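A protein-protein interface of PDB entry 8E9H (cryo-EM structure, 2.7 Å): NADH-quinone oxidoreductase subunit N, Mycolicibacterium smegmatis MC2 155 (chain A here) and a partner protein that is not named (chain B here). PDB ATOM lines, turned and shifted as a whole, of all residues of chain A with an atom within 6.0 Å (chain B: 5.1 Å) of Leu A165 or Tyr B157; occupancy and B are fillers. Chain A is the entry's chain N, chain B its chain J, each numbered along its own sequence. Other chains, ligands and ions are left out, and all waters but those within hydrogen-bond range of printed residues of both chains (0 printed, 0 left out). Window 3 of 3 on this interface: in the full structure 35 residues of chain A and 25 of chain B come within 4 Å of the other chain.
Of the 12 printed residues of chain A, 5 touch a printed residue of chain B. Among the printed residues, 6 pairs touch across the chains. Among the printed residues, no Asp or Glu carboxylate lies within 4 Å of a Lys or Arg side-chain nitrogen of the other chain.
Among the printed residues, merely in contact across the chains: Leu A224 with Tyr B157, Val A71 with Leu B158, Leu A165 with Tyr B157, Thr A166 with Trp B159, Val A71 with Thr B155 and Ala A74 with Arg B156.
Of chain B, only Tyr B157 (3.6 Å) comes within 4 Å of Leu A165. Of chain A, only Leu A165 and Leu A224 come within 4 Å of Tyr B157. Printed residues of chain B within 4 Å of Ala A74: Arg B156. Printed residues of chain B within 4 Å of Leu A224: Tyr B157 (3.2 Å). Printed residues of chain A within 4 Å of Trp B159: Thr A166. Printed residues of chain A within 4 Å of Thr B155: Val A71 (3.9 Å). Phe A168 touches none of the printed residues of chain B. Leu A164 touches none of the printed residues of chain B. The nearest residue of chain B that does not touch Leu A165 is Ala B160 (4.2 Å). The nearest printed residue of chain A that does not touch Thr B155 is Ala A74 (7.0 Å).
The backbone carbonyl oxygen (O) of Leu B152 is in hydrogen-bond range of the backbone NH (N) of Tyr B157 (3.0 Å). The backbone NH of Leu B158 lies within hydrogen-bond range of the backbone carbonyl oxygen of Ile B153 (2.8 Å). O of Ala A74 lies close to OG1 of Thr A166 (3.2 Å). N of Leu A164 is in hydrogen-bond range of O of Leu A224, 2.8 Å away.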
ATOM      1  N   VAL A  71     -24.822 -21.732 -16.003  1.00  0.00           N
ATOM      2  CA  VAL A  71     -24.367 -22.851 -15.184  1.00  0.00           C
ATOM      3  C   VAL A  71     -22.998 -22.530 -14.601  1.00  0.00           C
ATOM      4  O   VAL A  71     -22.144 -23.413 -14.474  1.00  0.00           O
ATOM      5  CB  VAL A  71     -24.328 -24.154 -16.002  1.00  0.00           C
ATOM      6  CG1 VAL A  71     -23.995 -25.340 -15.108  1.00  0.00           C
ATOM      7  CG2 VAL A  71     -25.650 -24.372 -16.718  1.00  0.00           C
ATOM      8  N   ALA A  74     -20.023 -21.786 -19.156  1.00  0.00           N
ATOM      9  CA  ALA A  74     -20.224 -23.071 -19.816  1.00  0.00           C
ATOM     10  C   ALA A  74     -21.537 -23.118 -20.589  1.00  0.00           C
ATOM     11  O   ALA A  74     -21.758 -24.039 -21.378  1.00  0.00           O
ATOM     12  CB  ALA A  74     -20.182 -24.206 -18.789  1.00  0.00           C
ATOM     13  N   ASP A 163     -18.262 -22.404 -23.399  1.00  0.00           N
ATOM     14  CA  ASP A 163     -16.965 -22.945 -23.029  1.00  0.00           C
ATOM     15  C   ASP A 163     -16.532 -23.967 -24.066  1.00  0.00           C
ATOM     16  O   ASP A 163     -17.363 -24.630 -24.691  1.00  0.00           O
ATOM     17  CB  ASP A 163     -17.005 -23.595 -21.644  1.00  0.00           C
ATOM     18  N   LEU A 164     -15.218 -24.091 -24.245  1.00  0.00           N
ATOM     19  CA  LEU A 164     -14.705 -25.039 -25.226  1.00  0.00           C
ATOM     20  C   LEU A 164     -15.134 -26.458 -24.888  1.00  0.00           C
ATOM     21  O   LEU A 164     -15.526 -27.223 -25.774  1.00  0.00           O
ATOM     22  CB  LEU A 164     -13.182 -24.948 -25.303  1.00  0.00           C
ATOM     23  CG  LEU A 164     -12.604 -23.935 -26.293  1.00  0.00           C
ATOM     24  CD1 LEU A 164     -12.994 -24.280 -27.717  1.00  0.00           C
ATOM     25  CD2 LEU A 164     -13.058 -22.540 -25.948  1.00  0.00           C
ATOM     26  N   LEU A 165     -15.066 -26.829 -23.610  1.00  0.00           N
ATOM     27  CA  LEU A 165     -15.441 -28.184 -23.221  1.00  0.00           C
ATOM     28  C   LEU A 165     -16.911 -28.449 -23.506  1.00  0.00           C
ATOM     29  O   LEU A 165     -17.268 -29.482 -24.084  1.00  0.00           O
ATOM     30  CB  LEU A 165     -15.140 -28.401 -21.741  1.00  0.00           C
ATOM     31  CG  LEU A 165     -15.679 -29.710 -21.167  1.00  0.00           C
ATOM     32  CD1 LEU A 165     -15.234 -30.886 -22.008  1.00  0.00           C
ATOM     33  CD2 LEU A 165     -15.232 -29.884 -19.733  1.00  0.00           C
ATOM     34  N   THR A 166     -17.783 -27.533 -23.092  1.00  0.00           N
ATOM     35  CA  THR A 166     -19.209 -27.731 -23.319  1.00  0.00           C
ATOM     36  C   THR A 166     -19.517 -27.786 -24.803  1.00  0.00           C
ATOM     37  O   THR A 166     -20.352 -28.580 -25.244  1.00  0.00           O
ATOM     38  CB  THR A 166     -20.010 -26.615 -22.660  1.00  0.00           C
ATOM     39  OG1 THR A 166     -19.555 -26.425 -21.317  1.00  0.00           O
ATOM     40  CG2 THR A 166     -21.484 -26.967 -22.650  1.00  0.00           C
ATOM     41  N   MET A 167     -18.862 -26.938 -25.589  1.00  0.00           N
ATOM     42  CA  MET A 167     -19.131 -26.908 -27.018  1.00  0.00           C
ATOM     43  C   MET A 167     -18.632 -28.179 -27.697  1.00  0.00           C
ATOM     44  O   MET A 167     -19.286 -28.699 -28.606  1.00  0.00           O
ATOM     45  CB  MET A 167     -18.511 -25.643 -27.608  1.00  0.00           C
ATOM     46  CG  MET A 167     -18.740 -25.420 -29.079  1.00  0.00           C
ATOM     47  SD  MET A 167     -17.989 -23.869 -29.605  1.00  0.00           S
ATOM     48  CE  MET A 167     -16.244 -24.247 -29.543  1.00  0.00           C
ATOM     49  N   PHE A 168     -17.500 -28.718 -27.244  1.00  0.00           N
ATOM     50  CA  PHE A 168     -17.045 -30.015 -27.741  1.00  0.00           C
ATOM     51  C   PHE A 168     -18.035 -31.114 -27.389  1.00  0.00           C
ATOM     52  O   PHE A 168     -18.349 -31.980 -28.217  1.00  0.00           O
ATOM     53  CB  PHE A 168     -15.677 -30.348 -27.158  1.00  0.00           C
ATOM     54  CG  PHE A 168     -15.200 -31.724 -27.500  1.00  0.00           C
ATOM     55  CD1 PHE A 168     -15.109 -32.133 -28.815  1.00  0.00           C
ATOM     56  CD2 PHE A 168     -14.858 -32.616 -26.502  1.00  0.00           C
ATOM     57  CE1 PHE A 168     -14.669 -33.400 -29.129  1.00  0.00           C
ATOM     58  CE2 PHE A 168     -14.420 -33.884 -26.812  1.00  0.00           C
ATOM     59  CZ  PHE A 168     -14.326 -34.276 -28.126  1.00  0.00           C
ATOM     60  N   VAL A 169     -18.521 -31.111 -26.149  1.00  0.00           N
ATOM     61  CA  VAL A 169     -19.470 -32.135 -25.733  1.00  0.00           C
ATOM     62  C   VAL A 169     -20.739 -32.037 -26.561  1.00  0.00           C
ATOM     63  O   VAL A 169     -21.318 -33.051 -26.957  1.00  0.00           O
ATOM     64  CB  VAL A 169     -19.762 -32.013 -24.229  1.00  0.00           C
ATOM     65  CG1 VAL A 169     -20.971 -32.845 -23.859  1.00  0.00           C
ATOM     66  CG2 VAL A 169     -18.556 -32.450 -23.429  1.00  0.00           C
ATOM     67  N   ALA A 170     -21.195 -30.815 -26.829  1.00  0.00           N
ATOM     68  CA  ALA A 170     -22.370 -30.631 -27.670  1.00  0.00           C
ATOM     69  C   ALA A 170     -22.115 -31.140 -29.079  1.00  0.00           C
ATOM     70  O   ALA A 170     -22.990 -31.761 -29.693  1.00  0.00           O
ATOM     71  CB  ALA A 170     -22.754 -29.158 -27.704  1.00  0.00           C
ATOM     72  N   ALA A 214      -9.172 -27.016 -29.273  1.00  0.00           N
ATOM     73  CA  ALA A 214      -9.571 -26.560 -27.950  1.00  0.00           C
ATOM     74  C   ALA A 214      -8.403 -26.645 -26.980  1.00  0.00           C
ATOM     75  O   ALA A 214      -8.203 -25.750 -26.154  1.00  0.00           O
ATOM     76  CB  ALA A 214     -10.751 -27.383 -27.441  1.00  0.00           C
ATOM     77  N   LEU A 224     -11.059 -22.056 -20.548  1.00  0.00           N
ATOM     78  CA  LEU A 224     -11.937 -22.693 -21.515  1.00  0.00           C
ATOM     79  C   LEU A 224     -13.146 -21.845 -21.874  1.00  0.00           C
ATOM     80  O   LEU A 224     -13.744 -22.067 -22.931  1.00  0.00           O
ATOM     81  CB  LEU A 224     -12.415 -24.043 -20.979  1.00  0.00           C
ATOM     82  CG  LEU A 224     -11.326 -25.111 -21.007  1.00  0.00           C
ATOM     83  CD1 LEU A 224     -11.574 -26.150 -19.940  1.00  0.00           C
ATOM     84  CD2 LEU A 224     -11.252 -25.754 -22.377  1.00  0.00           C
ATOM     85  N   LEU B 152     -14.246 -29.150  -9.628  1.00  0.00           N
ATOM     86  CA  LEU B 152     -14.418 -28.552 -10.949  1.00  0.00           C
ATOM     87  C   LEU B 152     -15.568 -29.204 -11.705  1.00  0.00           C
ATOM     88  O   LEU B 152     -16.417 -28.513 -12.278  1.00  0.00           O
ATOM     89  CB  LEU B 152     -13.123 -28.665 -11.749  1.00  0.00           C
ATOM     90  CG  LEU B 152     -12.227 -27.433 -11.702  1.00  0.00           C
ATOM     91  CD1 LEU B 152     -11.892 -27.071 -10.269  1.00  0.00           C
ATOM     92  CD2 LEU B 152     -10.966 -27.685 -12.499  1.00  0.00           C
ATOM     93  N   ILE B 153     -15.616 -30.535 -11.712  1.00  0.00           N
ATOM     94  CA  ILE B 153     -16.563 -31.245 -12.568  1.00  0.00           C
ATOM     95  C   ILE B 153     -17.994 -30.922 -12.168  1.00  0.00           C
ATOM     96  O   ILE B 153     -18.850 -30.656 -13.017  1.00  0.00           O
ATOM     97  CB  ILE B 153     -16.302 -32.760 -12.517  1.00  0.00           C
ATOM     98  CG1 ILE B 153     -15.024 -33.107 -13.277  1.00  0.00           C
ATOM     99  CG2 ILE B 153     -17.478 -33.515 -13.102  1.00  0.00           C
ATOM    100  CD1 ILE B 153     -14.486 -34.481 -12.962  1.00  0.00           C
ATOM    101  N   PHE B 154     -18.279 -30.950 -10.871  1.00  0.00           N
ATOM    102  CA  PHE B 154     -19.643 -30.837 -10.382  1.00  0.00           C
ATOM    103  C   PHE B 154     -20.024 -29.411 -10.022  1.00  0.00           C
ATOM    104  O   PHE B 154     -21.138 -29.183  -9.539  1.00  0.00           O
ATOM    105  CB  PHE B 154     -19.835 -31.771  -9.189  1.00  0.00           C
ATOM    106  CG  PHE B 154     -19.507 -33.194  -9.505  1.00  0.00           C
ATOM    107  CD1 PHE B 154     -20.335 -33.934 -10.325  1.00  0.00           C
ATOM    108  CD2 PHE B 154     -18.359 -33.780  -9.020  1.00  0.00           C
ATOM    109  CE1 PHE B 154     -20.035 -35.236 -10.635  1.00  0.00           C
ATOM    110  CE2 PHE B 154     -18.054 -35.084  -9.330  1.00  0.00           C
ATOM    111  CZ  PHE B 154     -18.891 -35.810 -10.142  1.00  0.00           C
ATOM    112  N   THR B 155     -19.129 -28.451 -10.237  1.00  0.00           N
ATOM    113  CA  THR B 155     -19.477 -27.046 -10.085  1.00  0.00           C
ATOM    114  C   THR B 155     -19.316 -26.307 -11.406  1.00  0.00           C
ATOM    115  O   THR B 155     -20.273 -25.716 -11.916  1.00  0.00           O
ATOM    116  CB  THR B 155     -18.609 -26.396  -9.010  1.00  0.00           C
ATOM    117  OG1 THR B 155     -17.230 -26.506  -9.378  1.00  0.00           O
ATOM    118  CG2 THR B 155     -18.829 -27.077  -7.671  1.00  0.00           C
ATOM    119  N   ARG B 156     -18.111 -26.348 -11.976  1.00  0.00           N
ATOM    120  CA  ARG B 156     -17.839 -25.572 -13.180  1.00  0.00           C
ATOM    121  C   ARG B 156     -18.332 -26.275 -14.433  1.00  0.00           C
ATOM    122  O   ARG B 156     -18.744 -25.615 -15.391  1.00  0.00           O
ATOM    123  CB  ARG B 156     -16.342 -25.292 -13.294  1.00  0.00           C
ATOM    124  N   TYR B 157     -18.287 -27.608 -14.456  1.00  0.00           N
ATOM    125  CA  TYR B 157     -18.610 -28.374 -15.654  1.00  0.00           C
ATOM    126  C   TYR B 157     -19.727 -29.380 -15.418  1.00  0.00           C
ATOM    127  O   TYR B 157     -19.748 -30.432 -16.061  1.00  0.00           O
ATOM    128  CB  TYR B 157     -17.368 -29.100 -16.169  1.00  0.00           C
ATOM    129  CG  TYR B 157     -16.205 -28.185 -16.435  1.00  0.00           C
ATOM    130  CD1 TYR B 157     -16.254 -27.252 -17.455  1.00  0.00           C
ATOM    131  CD2 TYR B 157     -15.058 -28.254 -15.664  1.00  0.00           C
ATOM    132  CE1 TYR B 157     -15.194 -26.414 -17.702  1.00  0.00           C
ATOM    133  CE2 TYR B 157     -13.994 -27.420 -15.903  1.00  0.00           C
ATOM    134  CZ  TYR B 157     -14.066 -26.502 -16.922  1.00  0.00           C
ATOM    135  OH  TYR B 157     -13.004 -25.666 -17.161  1.00  0.00           O
ATOM    136  N   LEU B 158     -20.659 -29.090 -14.511  1.00  0.00           N
ATOM    137  CA  LEU B 158     -21.737 -30.040 -14.270  1.00  0.00           C
ATOM    138  C   LEU B 158     -22.581 -30.240 -15.518  1.00  0.00           C
ATOM    139  O   LEU B 158     -23.138 -31.322 -15.724  1.00  0.00           O
ATOM    140  CB  LEU B 158     -22.610 -29.567 -13.110  1.00  0.00           C
ATOM    141  CG  LEU B 158     -23.338 -28.244 -13.331  1.00  0.00           C
ATOM    142  CD1 LEU B 158     -24.745 -28.486 -13.851  1.00  0.00           C
ATOM    143  CD2 LEU B 158     -23.372 -27.422 -12.057  1.00  0.00           C
ATOM    144  N   TRP B 159     -22.678 -29.218 -16.366  1.00  0.00           N
ATOM    145  CA  TRP B 159     -23.478 -29.341 -17.579  1.00  0.00           C
ATOM    146  C   TRP B 159     -22.889 -30.388 -18.517  1.00  0.00           C
ATOM    147  O   TRP B 159     -23.603 -31.272 -19.010  1.00  0.00           O
ATOM    148  CB  TRP B 159     -23.573 -27.982 -18.269  1.00  0.00           C
ATOM    149  CG  TRP B 159     -24.685 -27.898 -19.246  1.00  0.00           C
ATOM    150  CD1 TRP B 159     -24.581 -27.724 -20.589  1.00  0.00           C
ATOM    151  CD2 TRP B 159     -26.082 -27.997 -18.958  1.00  0.00           C
ATOM    152  NE1 TRP B 159     -25.828 -27.703 -21.161  1.00  0.00           N
ATOM    153  CE2 TRP B 159     -26.768 -27.869 -20.179  1.00  0.00           C
ATOM    154  CE3 TRP B 159     -26.819 -28.180 -17.787  1.00  0.00           C
ATOM    155  CZ2 TRP B 159     -28.154 -27.917 -20.264  1.00  0.00           C
ATOM    156  CZ3 TRP B 159     -28.194 -28.228 -17.872  1.00  0.00           C
ATOM    157  CH2 TRP B 159     -28.848 -28.098 -19.102  1.00  0.00           C
ATOM    158  N   ALA B 160     -21.583 -30.311 -18.769  1.00  0.00           N
ATOM    159  CA  ALA B 160     -20.934 -31.316 -19.599  1.00  0.00           C
ATOM    160  C   ALA B 160     -21.020 -32.690 -18.953  1.00  0.00           C
ATOM    161  O   ALA B 160     -21.199 -33.704 -19.640  1.00  0.00           O
ATOM    162  CB  ALA B 160     -19.478 -30.926 -19.842  1.00  0.00           C
ATOM    163  N   PHE B 161     -20.884 -32.745 -17.629  1.00  0.00           N
ATOM    164  CA  PHE B 161     -20.996 -34.012 -16.923  1.00  0.00           C
ATOM    165  C   PHE B 161     -22.352 -34.652 -17.186  1.00  0.00           C
ATOM    166  O   PHE B 161     -22.450 -35.850 -17.466  1.00  0.00           O
ATOM    167  CB  PHE B 161     -20.782 -33.791 -15.427  1.00  0.00           C
ATOM    168  CG  PHE B 161     -21.335 -34.884 -14.572  1.00  0.00           C
ATOM    169  CD1 PHE B 161     -20.871 -36.178 -14.696  1.00  0.00           C
ATOM    170  CD2 PHE B 161     -22.323 -34.619 -13.645  1.00  0.00           C
ATOM    171  CE1 PHE B 161     -21.380 -37.184 -13.912  1.00  0.00           C
ATOM    172  CE2 PHE B 161     -22.834 -35.623 -12.859  1.00  0.00           C
ATOM    173  CZ  PHE B 161     -22.363 -36.907 -12.993  1.00  0.00           C
